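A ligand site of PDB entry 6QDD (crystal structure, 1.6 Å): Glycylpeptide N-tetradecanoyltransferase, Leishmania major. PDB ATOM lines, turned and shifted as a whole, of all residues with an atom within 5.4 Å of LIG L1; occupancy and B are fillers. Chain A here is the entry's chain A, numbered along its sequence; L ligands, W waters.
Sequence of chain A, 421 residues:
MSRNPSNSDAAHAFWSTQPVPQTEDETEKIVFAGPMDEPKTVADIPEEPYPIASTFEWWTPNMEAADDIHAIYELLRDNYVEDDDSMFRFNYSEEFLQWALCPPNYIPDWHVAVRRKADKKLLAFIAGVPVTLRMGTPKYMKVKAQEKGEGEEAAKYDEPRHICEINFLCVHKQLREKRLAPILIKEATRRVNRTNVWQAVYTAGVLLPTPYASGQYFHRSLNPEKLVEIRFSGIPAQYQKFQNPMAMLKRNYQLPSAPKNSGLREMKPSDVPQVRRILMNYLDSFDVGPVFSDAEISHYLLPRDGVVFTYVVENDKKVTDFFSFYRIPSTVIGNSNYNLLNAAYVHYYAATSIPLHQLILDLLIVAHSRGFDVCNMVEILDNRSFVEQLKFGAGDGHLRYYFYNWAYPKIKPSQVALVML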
ATOM      1  N   TYR A  80      13.775 -14.312 -29.855  1.00  0.00           N
ATOM      2  CA  TYR A  80      12.640 -15.221 -30.019  1.00  0.00           C
ATOM      3  C   TYR A  80      11.446 -14.817 -29.132  1.00  0.00           C
ATOM      4  O   TYR A  80      11.317 -13.679 -28.684  1.00  0.00           O
ATOM      5  CB  TYR A  80      13.088 -16.687 -29.881  1.00  0.00           C
ATOM      6  CG  TYR A  80      12.173 -17.721 -30.506  1.00  0.00           C
ATOM      7  CD1 TYR A  80      11.688 -17.587 -31.801  1.00  0.00           C
ATOM      8  CD2 TYR A  80      11.824 -18.872 -29.780  1.00  0.00           C
ATOM      9  CE1 TYR A  80      10.864 -18.580 -32.343  1.00  0.00           C
ATOM     10  CE2 TYR A  80      11.020 -19.869 -30.310  1.00  0.00           C
ATOM     11  CZ  TYR A  80      10.557 -19.715 -31.609  1.00  0.00           C
ATOM     12  OH  TYR A  80       9.743 -20.694 -32.152  1.00  0.00           O
ATOM     13  N   VAL A  81      10.457 -15.719 -28.978  1.00  0.00           N
ATOM     14  CA  VAL A  81       9.159 -15.403 -28.395  1.00  0.00           C
ATOM     15  C   VAL A  81       9.307 -14.870 -26.955  1.00  0.00           C
ATOM     16  O   VAL A  81       9.969 -15.488 -26.124  1.00  0.00           O
ATOM     17  CB  VAL A  81       8.264 -16.678 -28.404  1.00  0.00           C
ATOM     18  CG1 VAL A  81       6.921 -16.448 -27.741  1.00  0.00           C
ATOM     19  CG2 VAL A  81       8.003 -17.159 -29.840  1.00  0.00           C
ATOM     20  N   PHE A  90      11.946 -17.046 -24.235  1.00  0.00           N
ATOM     21  CA  PHE A  90      12.484 -18.381 -24.294  1.00  0.00           C
ATOM     22  C   PHE A  90      13.978 -18.371 -24.577  1.00  0.00           C
ATOM     23  O   PHE A  90      14.458 -17.521 -25.359  1.00  0.00           O
ATOM     24  CB  PHE A  90      11.767 -19.206 -25.379  1.00  0.00           C
ATOM     25  CG  PHE A  90      10.330 -19.414 -24.996  1.00  0.00           C
ATOM     26  CD1 PHE A  90      10.020 -20.236 -23.935  1.00  0.00           C
ATOM     27  CD2 PHE A  90       9.304 -18.730 -25.650  1.00  0.00           C
ATOM     28  CE1 PHE A  90       8.701 -20.358 -23.523  1.00  0.00           C
ATOM     29  CE2 PHE A  90       7.989 -18.861 -25.238  1.00  0.00           C
ATOM     30  CZ  PHE A  90       7.682 -19.693 -24.178  1.00  0.00           C
ATOM     31  N   TYR A  92      15.866 -21.475 -25.542  1.00  0.00           N
ATOM     32  CA  TYR A  92      16.178 -22.835 -25.927  1.00  0.00           C
ATOM     33  C   TYR A  92      17.695 -23.024 -25.960  1.00  0.00           C
ATOM     34  O   TYR A  92      18.408 -22.191 -26.561  1.00  0.00           O
ATOM     35  CB  TYR A  92      15.646 -23.067 -27.338  1.00  0.00           C
ATOM     36  CG  TYR A  92      14.143 -23.218 -27.461  1.00  0.00           C
ATOM     37  CD1 TYR A  92      13.330 -22.115 -27.639  1.00  0.00           C
ATOM     38  CD2 TYR A  92      13.546 -24.487 -27.472  1.00  0.00           C
ATOM     39  CE1 TYR A  92      11.947 -22.229 -27.784  1.00  0.00           C
ATOM     40  CE2 TYR A  92      12.176 -24.615 -27.662  1.00  0.00           C
ATOM     41  CZ  TYR A  92      11.383 -23.495 -27.822  1.00  0.00           C
ATOM     42  OH  TYR A  92      10.032 -23.625 -28.036  1.00  0.00           O
ATOM     43  N   ASN A 167       9.154 -24.626 -37.362  1.00  0.00           N
ATOM     44  CA  ASN A 167       9.303 -24.077 -36.016  1.00  0.00           C
ATOM     45  C   ASN A 167      10.432 -23.061 -36.081  1.00  0.00           C
ATOM     46  O   ASN A 167      11.134 -22.896 -37.089  1.00  0.00           O
ATOM     47  CB  ASN A 167       9.624 -25.231 -35.040  1.00  0.00           C
ATOM     48  CG  ASN A 167       9.251 -24.974 -33.592  1.00  0.00           C
ATOM     49  OD1 ASN A 167       9.008 -23.845 -33.196  1.00  0.00           O
ATOM     50  ND2 ASN A 167       9.181 -26.021 -32.801  1.00  0.00           N
ATOM     51  N   THR A 203       2.715 -24.552 -35.302  1.00  0.00           N
ATOM     52  CA  THR A 203       1.874 -23.990 -34.249  1.00  0.00           C
ATOM     53  C   THR A 203       2.347 -22.569 -33.988  1.00  0.00           C
ATOM     54  O   THR A 203       3.479 -22.212 -34.327  1.00  0.00           O
ATOM     55  CB  THR A 203       1.952 -24.795 -32.955  1.00  0.00           C
ATOM     56  OG1 THR A 203       3.316 -24.910 -32.475  1.00  0.00           O
ATOM     57  CG2 THR A 203       1.327 -26.150 -33.146  1.00  0.00           C
ATOM     58  N   ALA A 204       1.450 -21.754 -33.424  1.00  0.00           N
ATOM     59  CA  ALA A 204       1.827 -20.422 -32.994  1.00  0.00           C
ATOM     60  C   ALA A 204       0.904 -20.004 -31.853  1.00  0.00           C
ATOM     61  O   ALA A 204      -0.249 -20.440 -31.762  1.00  0.00           O
ATOM     62  CB  ALA A 204       1.716 -19.446 -34.134  1.00  0.00           C
ATOM     63  N   GLY A 205       1.407 -19.050 -31.076  1.00  0.00           N
ATOM     64  CA  GLY A 205       0.613 -18.470 -30.024  1.00  0.00           C
ATOM     65  C   GLY A 205      -0.366 -17.471 -30.625  1.00  0.00           C
ATOM     66  O   GLY A 205      -1.465 -17.321 -30.111  1.00  0.00           O
ATOM     67  N   VAL A 206       0.019 -16.800 -31.733  1.00  0.00           N
ATOM     68  CA  VAL A 206      -0.805 -15.782 -32.375  1.00  0.00           C
ATOM     69  C   VAL A 206      -1.883 -16.447 -33.227  1.00  0.00           C
ATOM     70  O   VAL A 206      -1.721 -17.593 -33.681  1.00  0.00           O
ATOM     71  CB  VAL A 206      -0.013 -14.736 -33.178  1.00  0.00           C
ATOM     72  CG1 VAL A 206       0.870 -13.904 -32.229  1.00  0.00           C
ATOM     73  CG2 VAL A 206       0.848 -15.384 -34.270  1.00  0.00           C
ATOM     74  N   TYR A 217      -2.892 -23.196 -22.740  1.00  0.00           N
ATOM     75  CA  TYR A 217      -1.774 -23.607 -21.919  1.00  0.00           C
ATOM     76  C   TYR A 217      -2.157 -23.793 -20.465  1.00  0.00           C
ATOM     77  O   TYR A 217      -3.057 -23.104 -19.977  1.00  0.00           O
ATOM     78  CB  TYR A 217      -0.674 -22.536 -22.023  1.00  0.00           C
ATOM     79  CG  TYR A 217       0.270 -22.828 -23.162  1.00  0.00           C
ATOM     80  CD1 TYR A 217       1.281 -23.758 -22.999  1.00  0.00           C
ATOM     81  CD2 TYR A 217       0.163 -22.147 -24.364  1.00  0.00           C
ATOM     82  CE1 TYR A 217       2.174 -24.045 -24.021  1.00  0.00           C
ATOM     83  CE2 TYR A 217       1.063 -22.419 -25.401  1.00  0.00           C
ATOM     84  CZ  TYR A 217       2.057 -23.368 -25.206  1.00  0.00           C
ATOM     85  OH  TYR A 217       2.937 -23.672 -26.204  1.00  0.00           O
ATOM     86  N   PHE A 232       6.100 -14.643 -12.469  1.00  0.00           N
ATOM     87  CA  PHE A 232       5.440 -15.609 -13.326  1.00  0.00           C
ATOM     88  C   PHE A 232       4.059 -15.871 -12.751  1.00  0.00           C
ATOM     89  O   PHE A 232       3.079 -16.044 -13.489  1.00  0.00           O
ATOM     90  CB  PHE A 232       6.251 -16.902 -13.404  1.00  0.00           C
ATOM     91  CG  PHE A 232       5.581 -17.993 -14.208  1.00  0.00           C
ATOM     92  CD1 PHE A 232       4.721 -18.882 -13.610  1.00  0.00           C
ATOM     93  CD2 PHE A 232       5.810 -18.097 -15.568  1.00  0.00           C
ATOM     94  CE1 PHE A 232       4.075 -19.871 -14.355  1.00  0.00           C
ATOM     95  CE2 PHE A 232       5.197 -19.094 -16.319  1.00  0.00           C
ATOM     96  CZ  PHE A 232       4.323 -19.979 -15.704  1.00  0.00           C
ATOM     97  N   ILE A 328      12.640 -26.303 -21.393  1.00  0.00           N
ATOM     98  CA  ILE A 328      12.963 -25.056 -22.095  1.00  0.00           C
ATOM     99  C   ILE A 328      13.057 -23.987 -21.031  1.00  0.00           C
ATOM    100  O   ILE A 328      12.036 -23.662 -20.425  1.00  0.00           O
ATOM    101  CB  ILE A 328      11.913 -24.585 -23.136  1.00  0.00           C
ATOM    102  CG1 ILE A 328      11.552 -25.663 -24.167  1.00  0.00           C
ATOM    103  CG2 ILE A 328      12.440 -23.337 -23.816  1.00  0.00           C
ATOM    104  CD1 ILE A 328      10.276 -25.294 -24.931  1.00  0.00           C
ATOM    105  N   TYR A 345       8.238 -29.432 -19.813  1.00  0.00           N
ATOM    106  CA  TYR A 345       7.038 -29.513 -20.628  1.00  0.00           C
ATOM    107  C   TYR A 345       6.656 -30.960 -20.776  1.00  0.00           C
ATOM    108  O   TYR A 345       7.491 -31.780 -21.100  1.00  0.00           O
ATOM    109  CB  TYR A 345       7.369 -28.996 -22.027  1.00  0.00           C
ATOM    110  CG  TYR A 345       7.370 -27.492 -22.072  1.00  0.00           C
ATOM    111  CD1 TYR A 345       8.448 -26.777 -21.536  1.00  0.00           C
ATOM    112  CD2 TYR A 345       6.352 -26.806 -22.720  1.00  0.00           C
ATOM    113  CE1 TYR A 345       8.473 -25.380 -21.599  1.00  0.00           C
ATOM    114  CE2 TYR A 345       6.361 -25.417 -22.758  1.00  0.00           C
ATOM    115  CZ  TYR A 345       7.428 -24.727 -22.213  1.00  0.00           C
ATOM    116  OH  TYR A 345       7.440 -23.367 -22.294  1.00  0.00           O
ATOM    117  N   ASN A 376       4.773 -27.220 -17.744  1.00  0.00           N
ATOM    118  CA  ASN A 376       3.820 -26.632 -18.674  1.00  0.00           C
ATOM    119  C   ASN A 376       3.271 -27.734 -19.600  1.00  0.00           C
ATOM    120  O   ASN A 376       3.934 -28.762 -19.877  1.00  0.00           O
ATOM    121  CB  ASN A 376       4.513 -25.556 -19.532  1.00  0.00           C
ATOM    122  CG  ASN A 376       4.863 -24.343 -18.702  1.00  0.00           C
ATOM    123  OD1 ASN A 376       4.026 -23.825 -17.979  1.00  0.00           O
ATOM    124  ND2 ASN A 376       6.103 -23.906 -18.773  1.00  0.00           N
ATOM    125  N   GLY A 397      -2.520 -18.085 -22.207  1.00  0.00           N
ATOM    126  CA  GLY A 397      -2.226 -18.246 -23.628  1.00  0.00           C
ATOM    127  C   GLY A 397      -2.944 -19.430 -24.258  1.00  0.00           C
ATOM    128  O   GLY A 397      -3.411 -20.325 -23.542  1.00  0.00           O
ATOM    129  N   HIS A 398      -2.960 -19.426 -25.583  1.00  0.00           N
ATOM    130  CA  HIS A 398      -3.423 -20.590 -26.337  1.00  0.00           C
ATOM    131  C   HIS A 398      -2.328 -20.984 -27.321  1.00  0.00           C
ATOM    132  O   HIS A 398      -1.656 -20.107 -27.836  1.00  0.00           O
ATOM    133  CB  HIS A 398      -4.646 -20.230 -27.167  1.00  0.00           C
ATOM    134  CG  HIS A 398      -5.804 -19.886 -26.301  1.00  0.00           C
ATOM    135  ND1 HIS A 398      -5.940 -18.642 -25.702  1.00  0.00           N
ATOM    136  CD2 HIS A 398      -6.858 -20.624 -25.893  1.00  0.00           C
ATOM    137  CE1 HIS A 398      -7.049 -18.626 -24.976  1.00  0.00           C
ATOM    138  NE2 HIS A 398      -7.633 -19.807 -25.112  1.00  0.00           N
ATOM    139  N   LEU A 399      -2.212 -22.262 -27.636  1.00  0.00           N
ATOM    140  CA  LEU A 399      -1.412 -22.684 -28.784  1.00  0.00           C
ATOM    141  C   LEU A 399      -2.387 -23.048 -29.909  1.00  0.00           C
ATOM    142  O   LEU A 399      -3.343 -23.803 -29.676  1.00  0.00           O
ATOM    143  CB  LEU A 399      -0.525 -23.867 -28.410  1.00  0.00           C
ATOM    144  CG  LEU A 399       0.497 -24.260 -29.504  1.00  0.00           C
ATOM    145  CD1 LEU A 399       1.506 -23.143 -29.714  1.00  0.00           C
ATOM    146  CD2 LEU A 399       1.177 -25.591 -29.235  1.00  0.00           C
ATOM    147  N   MET A 420       4.439 -30.020 -30.082  1.00  0.00           N
ATOM    148  CA  MET A 420       5.383 -29.218 -30.837  1.00  0.00           C
ATOM    149  C   MET A 420       6.327 -28.526 -29.854  1.00  0.00           C
ATOM    150  O   MET A 420       5.888 -28.011 -28.850  1.00  0.00           O
ATOM    151  CB  MET A 420       4.666 -28.229 -31.763  1.00  0.00           C
ATOM    152  CG  MET A 420       4.094 -28.947 -33.005  1.00  0.00           C
ATOM    153  SD  MET A 420       4.385 -28.114 -34.580  1.00  0.00           S
ATOM    154  CE  MET A 420       6.023 -27.457 -34.314  1.00  0.00           C
ATOM    155  N   LEU A 421       7.616 -28.593 -30.158  1.00  0.00           N
ATOM    156  CA  LEU A 421       8.655 -28.162 -29.218  1.00  0.00           C
ATOM    157  C   LEU A 421       8.746 -26.628 -29.171  1.00  0.00           C
ATOM    158  O   LEU A 421       8.504 -25.915 -30.156  1.00  0.00           O
ATOM    159  CB  LEU A 421       9.983 -28.753 -29.681  1.00  0.00           C
ATOM    160  CG  LEU A 421      10.031 -30.263 -29.767  1.00  0.00           C
ATOM    161  CD1 LEU A 421      11.351 -30.721 -30.366  1.00  0.00           C
ATOM    162  CD2 LEU A 421       9.738 -30.945 -28.430  1.00  0.00           C
ATOM    163  OXT LEU A 421       9.103 -26.079 -28.120  1.00  0.00           O
HETATM  164  C1  LIG L   1       5.910 -22.008 -27.497  1.00  0.00           C
HETATM  165  C2  LIG L   1       7.188 -21.296 -28.001  1.00  0.00           C
HETATM  166  C3  LIG L   1       6.917 -20.692 -29.346  1.00  0.00           C
HETATM  167  N1  LIG L   1       6.281 -21.737 -30.163  1.00  0.00           N
HETATM  168  C4  LIG L   1       5.328 -21.863 -25.099  1.00  0.00           C
HETATM  169  C5  LIG L   1       5.753 -23.335 -28.237  1.00  0.00           C
HETATM  170  N2  LIG L   1       4.478 -20.903 -25.456  1.00  0.00           N
HETATM  171  C6  LIG L   1       5.806 -23.089 -29.764  1.00  0.00           C
HETATM  172  C7  LIG L   1       6.118 -21.335 -31.561  1.00  0.00           C
HETATM  173  C8  LIG L   1       3.613 -20.305 -24.629  1.00  0.00           C
HETATM  174  C9  LIG L   1       1.823 -18.656 -24.204  1.00  0.00           C
HETATM  175  N3  LIG L   1       4.380 -18.699 -30.014  1.00  0.00           N
HETATM  176  C10 LIG L   1       4.094 -18.619 -28.809  1.00  0.00           C
HETATM  177  C11 LIG L   1       3.832 -18.440 -27.300  1.00  0.00           C
HETATM  178  C12 LIG L   1       2.594 -19.095 -26.581  1.00  0.00           C
HETATM  179  C13 LIG L   1       1.326 -18.189 -26.548  1.00  0.00           C
HETATM  180  C14 LIG L   1       1.153 -17.659 -25.145  1.00  0.00           C
HETATM  181  N4  LIG L   1       2.744 -19.356 -25.111  1.00  0.00           N
HETATM  182  C15 LIG L   1       3.643 -20.811 -23.250  1.00  0.00           C
HETATM  183  C16 LIG L   1       4.592 -21.798 -22.875  1.00  0.00           C
HETATM  184  C17 LIG L   1       4.529 -22.201 -21.488  1.00  0.00           C
HETATM  185  C18 LIG L   1       3.529 -21.455 -20.790  1.00  0.00           C
HETATM  186  S1  LIG L   1       2.717 -20.375 -21.872  1.00  0.00           S
HETATM  187  N5  LIG L   1       5.469 -22.330 -23.834  1.00  0.00           N
HETATM  188  N6  LIG L   1       6.161 -22.377 -26.094  1.00  0.00           N
HETATM  189  C19 LIG L   1       7.259 -23.242 -25.731  1.00  0.00           C
HETATM  190  S1  LG2 L   2       5.628 -19.430 -34.238  1.00  0.00           S
HETATM  191  C1  LG2 L   2       6.972 -18.443 -33.471  1.00  0.00           C
HETATM  192  C2  LG2 L   2       7.120 -17.172 -34.279  1.00  0.00           C
HETATM  193  N1  LG2 L   2       8.267 -16.417 -33.785  1.00  0.00           N
HETATM  194  C3  LG2 L   2       8.169 -15.422 -32.881  1.00  0.00           C
HETATM  195  O1  LG2 L   2       7.078 -15.041 -32.414  1.00  0.00           O
HETATM  196  C4  LG2 L   2       9.499 -14.815 -32.510  1.00  0.00           C
HETATM  197  C5  LG2 L   2       9.483 -13.270 -32.258  1.00  0.00           C
HETATM  198  N2  LG2 L   2       8.816 -12.582 -33.391  1.00  0.00           N
HETATM  199  C6  LG2 L   2       9.451 -12.476 -34.559  1.00  0.00           C
HETATM  200  O2  LG2 L   2      10.610 -12.957 -34.692  1.00  0.00           O
HETATM  201  C7  LG2 L   2       8.766 -11.785 -35.702  1.00  0.00           C
HETATM  202  O3  LG2 L   2       7.769 -10.945 -35.120  1.00  0.00           O
HETATM  203  C8  LG2 L   2       8.042 -12.702 -36.722  1.00  0.00           C
HETATM  204  C9  LG2 L   2       7.197 -11.858 -37.652  1.00  0.00           C
HETATM  205  C10 LG2 L   2       7.121 -13.729 -35.996  1.00  0.00           C
HETATM  206  C11 LG2 L   2       9.099 -13.486 -37.494  1.00  0.00           C
HETATM  207  N3  LG2 L   2       3.708 -17.192 -38.097  1.00  0.00           N
HETATM  208  O4  LG2 L   2       8.306  -9.626 -41.345  1.00  0.00           O
HETATM  209  P1  LG2 L   2       6.988  -9.086 -41.063  1.00  0.00           P
HETATM  210  C12 LG2 L   2       2.883 -12.660 -40.399  1.00  0.00           C
HETATM  211  C13 LG2 L   2       3.397 -16.938 -39.402  1.00  0.00           C
HETATM  212  O5  LG2 L   2       6.749  -7.654 -41.446  1.00  0.00           O
HETATM  213  P2  LG2 L   2       7.744  -9.382 -38.277  1.00  0.00           P
HETATM  214  C14 LG2 L   2       6.490 -20.365 -35.391  1.00  0.00           C
HETATM  215  O6  LG2 L   2       7.715 -20.399 -35.383  1.00  0.00           O
HETATM  216  C15 LG2 L   2       1.900 -11.525 -40.210  1.00  0.00           C
HETATM  217  O7  LG2 L   2       0.545 -11.986 -40.097  1.00  0.00           O
HETATM  218  N4  LG2 L   2       3.192 -15.661 -39.846  1.00  0.00           N
HETATM  219  O8  LG2 L   2       6.657  -9.241 -39.431  1.00  0.00           O
HETATM  220  C16 LG2 L   2       5.622 -21.003 -36.431  1.00  0.00           C
HETATM  221  C17 LG2 L   2       2.180 -10.799 -41.480  1.00  0.00           C
HETATM  222  O9  LG2 L   2       1.440 -11.363 -42.587  1.00  0.00           O
HETATM  223  P3  LG2 L   2       0.075 -10.708 -43.137  1.00  0.00           P
HETATM  224  C18 LG2 L   2       3.341 -14.636 -38.957  1.00  0.00           C
HETATM  225  O10 LG2 L   2       6.998  -9.073 -37.030  1.00  0.00           O
HETATM  226  C19 LG2 L   2       5.891 -20.287 -37.785  1.00  0.00           C
HETATM  227  C20 LG2 L   2       3.631 -10.970 -41.711  1.00  0.00           C
HETATM  228  O11 LG2 L   2       4.073 -12.081 -40.865  1.00  0.00           O
HETATM  229  C21 LG2 L   2       3.682 -14.868 -37.650  1.00  0.00           C
HETATM  230  O12 LG2 L   2       9.006  -8.637 -38.535  1.00  0.00           O
HETATM  231  C22 LG2 L   2       4.977 -20.810 -38.919  1.00  0.00           C
HETATM  232  C23 LG2 L   2       4.401  -9.717 -41.371  1.00  0.00           C
HETATM  233  O13 LG2 L   2       5.784  -9.970 -41.560  1.00  0.00           O
HETATM  234  C24 LG2 L   2       3.869 -16.183 -37.217  1.00  0.00           C
HETATM  235  N5  LG2 L   2       4.222 -16.453 -35.926  1.00  0.00           N
HETATM  236  O14 LG2 L   2       8.106 -10.949 -38.274  1.00  0.00           O
HETATM  237  C25 LG2 L   2       5.341 -20.008 -40.197  1.00  0.00           C
HETATM  238  N6  LG2 L   2       3.773 -13.647 -36.998  1.00  0.00           N
HETATM  239  O15 LG2 L   2      -0.895 -10.718 -41.948  1.00  0.00           O
HETATM  240  C26 LG2 L   2       4.450 -20.434 -41.372  1.00  0.00           C
HETATM  241  C27 LG2 L   2       3.513 -12.686 -37.931  1.00  0.00           C
HETATM  242  O16 LG2 L   2       0.513  -9.338 -43.530  1.00  0.00           O
HETATM  243  C28 LG2 L   2       5.019 -21.714 -41.996  1.00  0.00           C
HETATM  244  N7  LG2 L   2       3.229 -13.308 -39.117  1.00  0.00           N
HETATM  245  O17 LG2 L   2      -0.514 -11.647 -44.187  1.00  0.00           O
HETATM  246  C29 LG2 L   2       4.151 -22.052 -43.241  1.00  0.00           C
HETATM  247  C30 LG2 L   2       4.584 -23.426 -43.883  1.00  0.00           C
HETATM  248  C31 LG2 L   2       5.827 -23.180 -44.750  1.00  0.00           C
HETATM  249  C32 LG2 L   2       6.334 -24.516 -45.370  1.00  0.00           C
HETATM  250  C33 LG2 L   2       5.359 -25.097 -46.449  1.00  0.00           C
HETATM  251  C34 LG2 L   2       5.921 -26.427 -47.007  1.00  0.00           C
HETATM  252  C35 LG2 L   2       4.810 -27.173 -47.795  1.00  0.00           C
HETATM  253  O   HOH W   1       4.278 -26.134 -29.715  1.00  0.00           O
HETATM  254  O   HOH W   2       3.109 -16.635 -31.709  1.00  0.00           O
HETATM  255  O   HOH W   3      -0.195 -19.234 -20.829  1.00  0.00           O
HETATM  256  O   HOH W   4       9.141 -22.888 -30.616  1.00  0.00           O
HETATM  257  O   HOH W   5       3.122 -15.364 -29.061  1.00  0.00           O
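Tyr 80 touches LIG L1. Val 81 touches LIG L1. Phe 90 touches LIG L1. Tyr 92 touches LIG L1. Thr 203 touches LIG L1. Ile 328 touches LIG L1 (CD1 to C19, 3.7 Å). CG of Asn 376 touches C17 of LIG L1, at 3.5 Å. Gly 397 touches LIG L1. His 398 touches LIG L1 (O to C13, 3.8 Å). Leu 421 touches LIG L1 (O to C6, 3.9 Å). Of the 19 residues printed, 13 come within 4 Å of LIG L1.
OXT of Leu 421 sits at hydrogen-bond distance from OH of Tyr 92 (2.6 Å). OD1 of Asn 167 is in hydrogen-bond range of OH of Tyr 80 (3.4 Å). O of Gly 397 is in hydrogen-bond range of N of Tyr 217 (3.0 Å). The chain-end carboxylate of Leu 421 lies within hydrogen-bond range of the side-chain amide nitrogen of Asn 167. N of Phe 90 is in hydrogen-bond range of O of Val 81 (3.1 Å).
Water W2 lies within hydrogen-bond range of N3 of LIG L1 (3.0 Å), N of Gly 205 (3.0 Å) and N of Val 206 (3.1 Å). Water W4 lies within hydrogen-bond range of OH of Tyr 80, OD1 of Asn 167, OH of Tyr 92 and O of Leu 421. Water W3 lies within hydrogen-bond range of N of Gly 397 and S1 of LIG L1. Water W1 lies within hydrogen-bond range of O of Met 420 (2.6 Å) and OG1 of Thr 203 (3.2 Å).
The backbone NH (N) of Gly 205 is in hydrogen-bond range of a nitrogen (N3) of LIG L1 (3.2 Å). OH of Tyr 217 sits close to N2 of LIG L1. OH of Tyr 345 sits at hydrogen-bond distance from N5 of LIG L1 (2.7 Å).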
